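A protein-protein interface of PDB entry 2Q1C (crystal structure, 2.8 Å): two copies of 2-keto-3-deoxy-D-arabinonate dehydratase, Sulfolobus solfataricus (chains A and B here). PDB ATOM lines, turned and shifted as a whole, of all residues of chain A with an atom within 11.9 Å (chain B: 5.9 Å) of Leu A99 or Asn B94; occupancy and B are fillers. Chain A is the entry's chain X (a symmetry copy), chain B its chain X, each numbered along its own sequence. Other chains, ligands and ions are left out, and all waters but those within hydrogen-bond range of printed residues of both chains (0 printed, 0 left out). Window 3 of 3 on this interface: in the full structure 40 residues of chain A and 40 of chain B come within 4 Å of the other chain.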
ATOM      1  N   ASN A  94      -1.840  25.506  14.226  1.00  0.00           N
ATOM      2  CA  ASN A  94      -2.142  24.629  13.091  1.00  0.00           C
ATOM      3  C   ASN A  94      -1.686  25.187  11.736  1.00  0.00           C
ATOM      4  O   ASN A  94      -1.452  26.390  11.589  1.00  0.00           O
ATOM      5  CB  ASN A  94      -3.632  24.233  13.067  1.00  0.00           C
ATOM      6  CG  ASN A  94      -4.565  25.431  12.972  1.00  0.00           C
ATOM      7  OD1 ASN A  94      -4.869  25.912  11.878  1.00  0.00           O
ATOM      8  ND2 ASN A  94      -5.040  25.903  14.120  1.00  0.00           N
ATOM      9  N   VAL A  95      -1.528  24.288  10.767  1.00  0.00           N
ATOM     10  CA  VAL A  95      -1.354  24.669   9.370  1.00  0.00           C
ATOM     11  C   VAL A  95      -2.721  24.650   8.681  1.00  0.00           C
ATOM     12  O   VAL A  95      -3.755  24.644   9.355  1.00  0.00           O
ATOM     13  CB  VAL A  95      -0.339  23.756   8.632  1.00  0.00           C
ATOM     14  CG1 VAL A  95       1.082  24.256   8.846  1.00  0.00           C
ATOM     15  CG2 VAL A  95      -0.484  22.299   9.068  1.00  0.00           C
ATOM     16  N   ALA A  96      -2.728  24.649   7.350  1.00  0.00           N
ATOM     17  CA  ALA A  96      -3.976  24.627   6.589  1.00  0.00           C
ATOM     18  C   ALA A  96      -4.643  23.257   6.670  1.00  0.00           C
ATOM     19  O   ALA A  96      -4.051  22.242   6.290  1.00  0.00           O
ATOM     20  CB  ALA A  96      -3.728  25.024   5.140  1.00  0.00           C
ATOM     21  N   LYS A  97      -5.873  23.233   7.181  1.00  0.00           N
ATOM     22  CA  LYS A  97      -6.621  21.984   7.326  1.00  0.00           C
ATOM     23  C   LYS A  97      -8.076  22.072   6.859  1.00  0.00           C
ATOM     24  O   LYS A  97      -8.810  22.996   7.225  1.00  0.00           O
ATOM     25  CB  LYS A  97      -6.521  21.433   8.759  1.00  0.00           C
ATOM     26  CG  LYS A  97      -6.826  22.432   9.875  1.00  0.00           C
ATOM     27  CD  LYS A  97      -6.154  22.024  11.188  1.00  0.00           C
ATOM     28  CE  LYS A  97      -6.805  20.792  11.811  1.00  0.00           C
ATOM     29  NZ  LYS A  97      -5.977  20.220  12.909  1.00  0.00           N
ATOM     30  N   ILE A  98      -8.463  21.101   6.035  1.00  0.00           N
ATOM     31  CA  ILE A  98      -9.821  20.987   5.507  1.00  0.00           C
ATOM     32  C   ILE A  98     -10.547  19.848   6.223  1.00  0.00           C
ATOM     33  O   ILE A  98     -10.130  18.686   6.146  1.00  0.00           O
ATOM     34  CB  ILE A  98      -9.822  20.740   3.971  1.00  0.00           C
ATOM     35  CG1 ILE A  98      -9.056  21.851   3.240  1.00  0.00           C
ATOM     36  CG2 ILE A  98     -11.255  20.621   3.436  1.00  0.00           C
ATOM     37  CD1 ILE A  98      -8.683  21.515   1.806  1.00  0.00           C
ATOM     38  N   LEU A  99     -11.630  20.201   6.917  1.00  0.00           N
ATOM     39  CA  LEU A  99     -12.447  19.255   7.693  1.00  0.00           C
ATOM     40  C   LEU A  99     -11.657  18.496   8.769  1.00  0.00           C
ATOM     41  O   LEU A  99     -11.915  17.317   9.031  1.00  0.00           O
ATOM     42  CB  LEU A  99     -13.214  18.281   6.768  1.00  0.00           C
ATOM     43  CG  LEU A  99     -14.568  18.645   6.127  1.00  0.00           C
ATOM     44  CD1 LEU A  99     -15.646  18.933   7.177  1.00  0.00           C
ATOM     45  CD2 LEU A  99     -14.476  19.793   5.116  1.00  0.00           C
ATOM     46  N   GLY A 100     -10.696  19.183   9.388  1.00  0.00           N
ATOM     47  CA  GLY A 100      -9.901  18.611  10.476  1.00  0.00           C
ATOM     48  C   GLY A 100      -8.634  17.897  10.036  1.00  0.00           C
ATOM     49  O   GLY A 100      -7.714  17.705  10.834  1.00  0.00           O
ATOM     50  N   LYS A 101      -8.592  17.494   8.768  1.00  0.00           N
ATOM     51  CA  LYS A 101      -7.423  16.840   8.188  1.00  0.00           C
ATOM     52  C   LYS A 101      -6.585  17.880   7.446  1.00  0.00           C
ATOM     53  O   LYS A 101      -7.132  18.724   6.733  1.00  0.00           O
ATOM     54  CB  LYS A 101      -7.865  15.730   7.233  1.00  0.00           C
ATOM     55  CG  LYS A 101      -6.900  14.566   7.143  1.00  0.00           C
ATOM     56  CD  LYS A 101      -7.380  13.505   6.168  1.00  0.00           C
ATOM     57  CE  LYS A 101      -6.439  12.307   6.158  1.00  0.00           C
ATOM     58  NZ  LYS A 101      -6.793  11.327   5.096  1.00  0.00           N
ATOM     59  N   THR A 102      -5.264  17.822   7.621  1.00  0.00           N
ATOM     60  CA  THR A 102      -4.362  18.813   7.021  1.00  0.00           C
ATOM     61  C   THR A 102      -4.237  18.634   5.501  1.00  0.00           C
ATOM     62  O   THR A 102      -4.337  17.515   4.988  1.00  0.00           O
ATOM     63  CB  THR A 102      -2.970  18.851   7.726  1.00  0.00           C
ATOM     64  OG1 THR A 102      -2.403  20.159   7.596  1.00  0.00           O
ATOM     65  CG2 THR A 102      -1.999  17.827   7.146  1.00  0.00           C
ATOM     66  N   ILE A 103      -4.021  19.743   4.795  1.00  0.00           N
ATOM     67  CA  ILE A 103      -3.973  19.745   3.325  1.00  0.00           C
ATOM     68  C   ILE A 103      -2.910  18.810   2.747  1.00  0.00           C
ATOM     69  O   ILE A 103      -3.092  18.248   1.666  1.00  0.00           O
ATOM     70  CB  ILE A 103      -3.800  21.177   2.730  1.00  0.00           C
ATOM     71  CG1 ILE A 103      -2.531  21.855   3.261  1.00  0.00           C
ATOM     72  CG2 ILE A 103      -5.040  22.027   2.999  1.00  0.00           C
ATOM     73  CD1 ILE A 103      -2.023  22.994   2.392  1.00  0.00           C
ATOM     74  N   TYR A 104      -1.813  18.642   3.481  1.00  0.00           N
ATOM     75  CA  TYR A 104      -0.702  17.803   3.042  1.00  0.00           C
ATOM     76  C   TYR A 104      -1.023  16.312   3.158  1.00  0.00           C
ATOM     77  O   TYR A 104      -0.679  15.530   2.269  1.00  0.00           O
ATOM     78  CB  TYR A 104       0.584  18.161   3.800  1.00  0.00           C
ATOM     79  CG  TYR A 104       1.025  19.598   3.598  1.00  0.00           C
ATOM     80  CD1 TYR A 104       1.747  19.973   2.467  1.00  0.00           C
ATOM     81  CD2 TYR A 104       0.714  20.581   4.535  1.00  0.00           C
ATOM     82  CE1 TYR A 104       2.147  21.288   2.270  1.00  0.00           C
ATOM     83  CE2 TYR A 104       1.113  21.902   4.349  1.00  0.00           C
ATOM     84  CZ  TYR A 104       1.829  22.245   3.215  1.00  0.00           C
ATOM     85  OH  TYR A 104       2.226  23.547   3.023  1.00  0.00           O
ATOM     86  N   GLU A 105      -1.688  15.920   4.243  1.00  0.00           N
ATOM     87  CA  GLU A 105      -2.089  14.522   4.414  1.00  0.00           C
ATOM     88  C   GLU A 105      -3.341  14.174   3.600  1.00  0.00           C
ATOM     89  O   GLU A 105      -3.656  12.998   3.408  1.00  0.00           O
ATOM     90  CB  GLU A 105      -2.233  14.145   5.898  1.00  0.00           C
ATOM     91  CG  GLU A 105      -3.402  14.777   6.639  1.00  0.00           C
ATOM     92  CD  GLU A 105      -3.271  14.676   8.159  1.00  0.00           C
ATOM     93  OE1 GLU A 105      -2.296  14.055   8.647  1.00  0.00           O
ATOM     94  OE2 GLU A 105      -4.143  15.226   8.869  1.00  0.00           O
ATOM     95  N   LYS A 106      -4.040  15.203   3.121  1.00  0.00           N
ATOM     96  CA  LYS A 106      -5.121  15.030   2.152  1.00  0.00           C
ATOM     97  C   LYS A 106      -4.580  14.568   0.799  1.00  0.00           C
ATOM     98  O   LYS A 106      -5.065  13.584   0.237  1.00  0.00           O
ATOM     99  CB  LYS A 106      -5.913  16.326   1.976  1.00  0.00           C
ATOM    100  CG  LYS A 106      -7.236  16.353   2.711  1.00  0.00           C
ATOM    101  CD  LYS A 106      -8.226  17.260   1.997  1.00  0.00           C
ATOM    102  CE  LYS A 106      -9.663  16.847   2.289  1.00  0.00           C
ATOM    103  NZ  LYS A 106     -10.632  17.572   1.423  1.00  0.00           N
ATOM    104  N   VAL A 107      -3.572  15.282   0.297  1.00  0.00           N
ATOM    105  CA  VAL A 107      -2.953  14.997  -1.003  1.00  0.00           C
ATOM    106  C   VAL A 107      -2.252  13.636  -1.029  1.00  0.00           C
ATOM    107  O   VAL A 107      -2.262  12.947  -2.052  1.00  0.00           O
ATOM    108  CB  VAL A 107      -1.973  16.129  -1.425  1.00  0.00           C
ATOM    109  CG1 VAL A 107      -1.182  15.746  -2.671  1.00  0.00           C
ATOM    110  CG2 VAL A 107      -2.733  17.422  -1.671  1.00  0.00           C
ATOM    111  N   ASP A 109      -3.248  10.998   0.413  1.00  0.00           N
ATOM    112  CA  ASP A 109      -4.316  10.011   0.242  1.00  0.00           C
ATOM    113  C   ASP A 109      -5.064  10.138  -1.086  1.00  0.00           C
ATOM    114  O   ASP A 109      -5.410   9.127  -1.698  1.00  0.00           O
ATOM    115  CB  ASP A 109      -5.321  10.109   1.395  1.00  0.00           C
ATOM    116  CG  ASP A 109      -4.761   9.597   2.708  1.00  0.00           C
ATOM    117  OD1 ASP A 109      -4.189   8.483   2.725  1.00  0.00           O
ATOM    118  OD2 ASP A 109      -4.905  10.307   3.729  1.00  0.00           O
ATOM    119  N   GLU B  92     -18.050  27.753   1.519  1.00  0.00           N
ATOM    120  CA  GLU B  92     -18.516  26.461   2.030  1.00  0.00           C
ATOM    121  C   GLU B  92     -17.700  25.977   3.228  1.00  0.00           C
ATOM    122  O   GLU B  92     -16.491  26.216   3.304  1.00  0.00           O
ATOM    123  CB  GLU B  92     -18.494  25.403   0.918  1.00  0.00           C
ATOM    124  CG  GLU B  92     -19.509  25.627  -0.206  1.00  0.00           C
ATOM    125  CD  GLU B  92     -20.939  25.305   0.206  1.00  0.00           C
ATOM    126  OE1 GLU B  92     -21.161  24.258   0.854  1.00  0.00           O
ATOM    127  OE2 GLU B  92     -21.846  26.098  -0.130  1.00  0.00           O
ATOM    128  N   GLU B  93     -18.377  25.303   4.159  1.00  0.00           N
ATOM    129  CA  GLU B  93     -17.745  24.753   5.360  1.00  0.00           C
ATOM    130  C   GLU B  93     -17.305  23.295   5.181  1.00  0.00           C
ATOM    131  O   GLU B  93     -18.139  22.389   5.128  1.00  0.00           O
ATOM    132  CB  GLU B  93     -18.662  24.900   6.583  1.00  0.00           C
ATOM    133  CG  GLU B  93     -18.293  26.041   7.535  1.00  0.00           C
ATOM    134  CD  GLU B  93     -18.443  27.422   6.913  1.00  0.00           C
ATOM    135  OE1 GLU B  93     -17.530  27.852   6.170  1.00  0.00           O
ATOM    136  OE2 GLU B  93     -19.466  28.087   7.182  1.00  0.00           O
ATOM    137  N   ASN B  94     -15.994  23.074   5.079  1.00  0.00           N
ATOM    138  CA  ASN B  94     -15.010  24.160   5.102  1.00  0.00           C
ATOM    139  C   ASN B  94     -13.954  24.066   3.994  1.00  0.00           C
ATOM    140  O   ASN B  94     -13.738  23.000   3.408  1.00  0.00           O
ATOM    141  CB  ASN B  94     -14.359  24.299   6.494  1.00  0.00           C
ATOM    142  CG  ASN B  94     -13.646  23.035   6.946  1.00  0.00           C
ATOM    143  OD1 ASN B  94     -12.474  22.818   6.627  1.00  0.00           O
ATOM    144  ND2 ASN B  94     -14.345  22.203   7.711  1.00  0.00           N
ATOM    145  N   VAL B  95     -13.332  25.204   3.692  1.00  0.00           N
ATOM    146  CA  VAL B  95     -12.136  25.242   2.858  1.00  0.00           C
ATOM    147  C   VAL B  95     -10.902  25.220   3.765  1.00  0.00           C
ATOM    148  O   VAL B  95     -11.007  24.877   4.946  1.00  0.00           O
ATOM    149  CB  VAL B  95     -12.116  26.472   1.912  1.00  0.00           C
ATOM    150  CG1 VAL B  95     -12.884  26.172   0.632  1.00  0.00           C
ATOM    151  CG2 VAL B  95     -12.666  27.716   2.607  1.00  0.00           C
ATOM    152  N   ALA B  96      -9.742  25.574   3.217  1.00  0.00           N
ATOM    153  CA  ALA B  96      -8.502  25.594   3.992  1.00  0.00           C
ATOM    154  C   ALA B  96      -8.486  26.765   4.971  1.00  0.00           C
ATOM    155  O   ALA B  96      -8.598  27.927   4.568  1.00  0.00           O
ATOM    156  CB  ALA B  96      -7.293  25.643   3.068  1.00  0.00           C
ATOM    157  N   LYS B  97      -8.361  26.450   6.259  1.00  0.00           N
ATOM    158  CA  LYS B  97      -8.343  27.476   7.302  1.00  0.00           C
ATOM    159  C   LYS B  97      -7.244  27.278   8.349  1.00  0.00           C
ATOM    160  O   LYS B  97      -7.068  26.184   8.894  1.00  0.00           O
ATOM    161  CB  LYS B  97      -9.725  27.634   7.958  1.00  0.00           C
ATOM    162  CG  LYS B  97     -10.390  26.338   8.421  1.00  0.00           C
ATOM    163  CD  LYS B  97     -11.911  26.486   8.492  1.00  0.00           C
ATOM    164  CE  LYS B  97     -12.351  27.384   9.646  1.00  0.00           C
ATOM    165  NZ  LYS B  97     -13.785  27.770   9.536  1.00  0.00           N
ATOM    166  N   ALA B 172     -11.113  24.321  -4.941  1.00  0.00           N
ATOM    167  CA  ALA B 172     -11.964  24.088  -3.774  1.00  0.00           C
ATOM    168  C   ALA B 172     -11.677  22.735  -3.129  1.00  0.00           C
ATOM    169  O   ALA B 172     -11.792  22.581  -1.912  1.00  0.00           O
ATOM    170  CB  ALA B 172     -13.429  24.186  -4.167  1.00  0.00           C
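Among the printed residues, pairs that only touch across the chains: Ile A98 with Asn B94, Lys A97 with Lys B97, Lys A97 with Val B95, Val A95 with Lys B97, Asn A94 with Lys B97, Lys A97 with Asn B94, Ile A98 with Ala B96 and Ile A98 with Val B95.
Of the printed residues of chain B, Asn A94 touches Lys B97 (3.7 Å). Printed residues of chain B within 4 Å of Val A95: Lys B97. Ala A96 touches none of the printed residues of chain B. Of the printed residues of chain B, Lys A97 touches Asn B94 (3.7 Å), Val B95 (3.7 Å) and Lys B97 (3.6 Å). Printed residues of chain B within 4 Å of Ile A98: Asn B94, Val B95 and Ala B96. Of chain B, only Asn B94 (2.8 Å) comes within 4 Å of Leu A99. Thr A102 touches none of the printed residues of chain B. No residue of chain A comes within 4 Å of Glu B93. Of chain A, only Lys A97 and Ile A98 come within 4 Å of Val B95. Of chain A, only Ile A98 (3.8 Å) comes within 4 Å of Ala B96. The nearest residue of chain A that does not touch Asn B94 is Gly A100 (4.9 Å). The nearest printed residue of chain B that does not touch Ile A98 is Ala B172 (5.0 Å).
Printed residues of chain B that touch a printed residue of chain A: Asn B94, Val B95, Ala B96 and Lys B97. Printed residues of chain A that touch a printed residue of chain B: Asn A94, Val A95, Lys A97, Ile A98 and Leu A99. Hydrophobic or aromatic side chains of chain A that line the printed part of chain B: Ile A98 and Leu A99. Among the printed residues, no Asp or Glu carboxylate lies within 4 Å of a Lys or Arg side-chain nitrogen of the other chain.
OD1 of Asn B94 sits at hydrogen-bond distance from N of Leu A99 (2.8 Å).
Asn A94 touches Lys B97, and with the chains exchanged Lys A97 touches Asn B94. Val A95 touches Lys B97, and with the chains exchanged Lys A97 touches Val B95. Lys B97 touches its own counterpart, Lys A97. 4 positions are printed for both chains. Of the 9 pairs that touch across the chains among the printed residues, 5 have their exchanged pair printed and touching as well.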
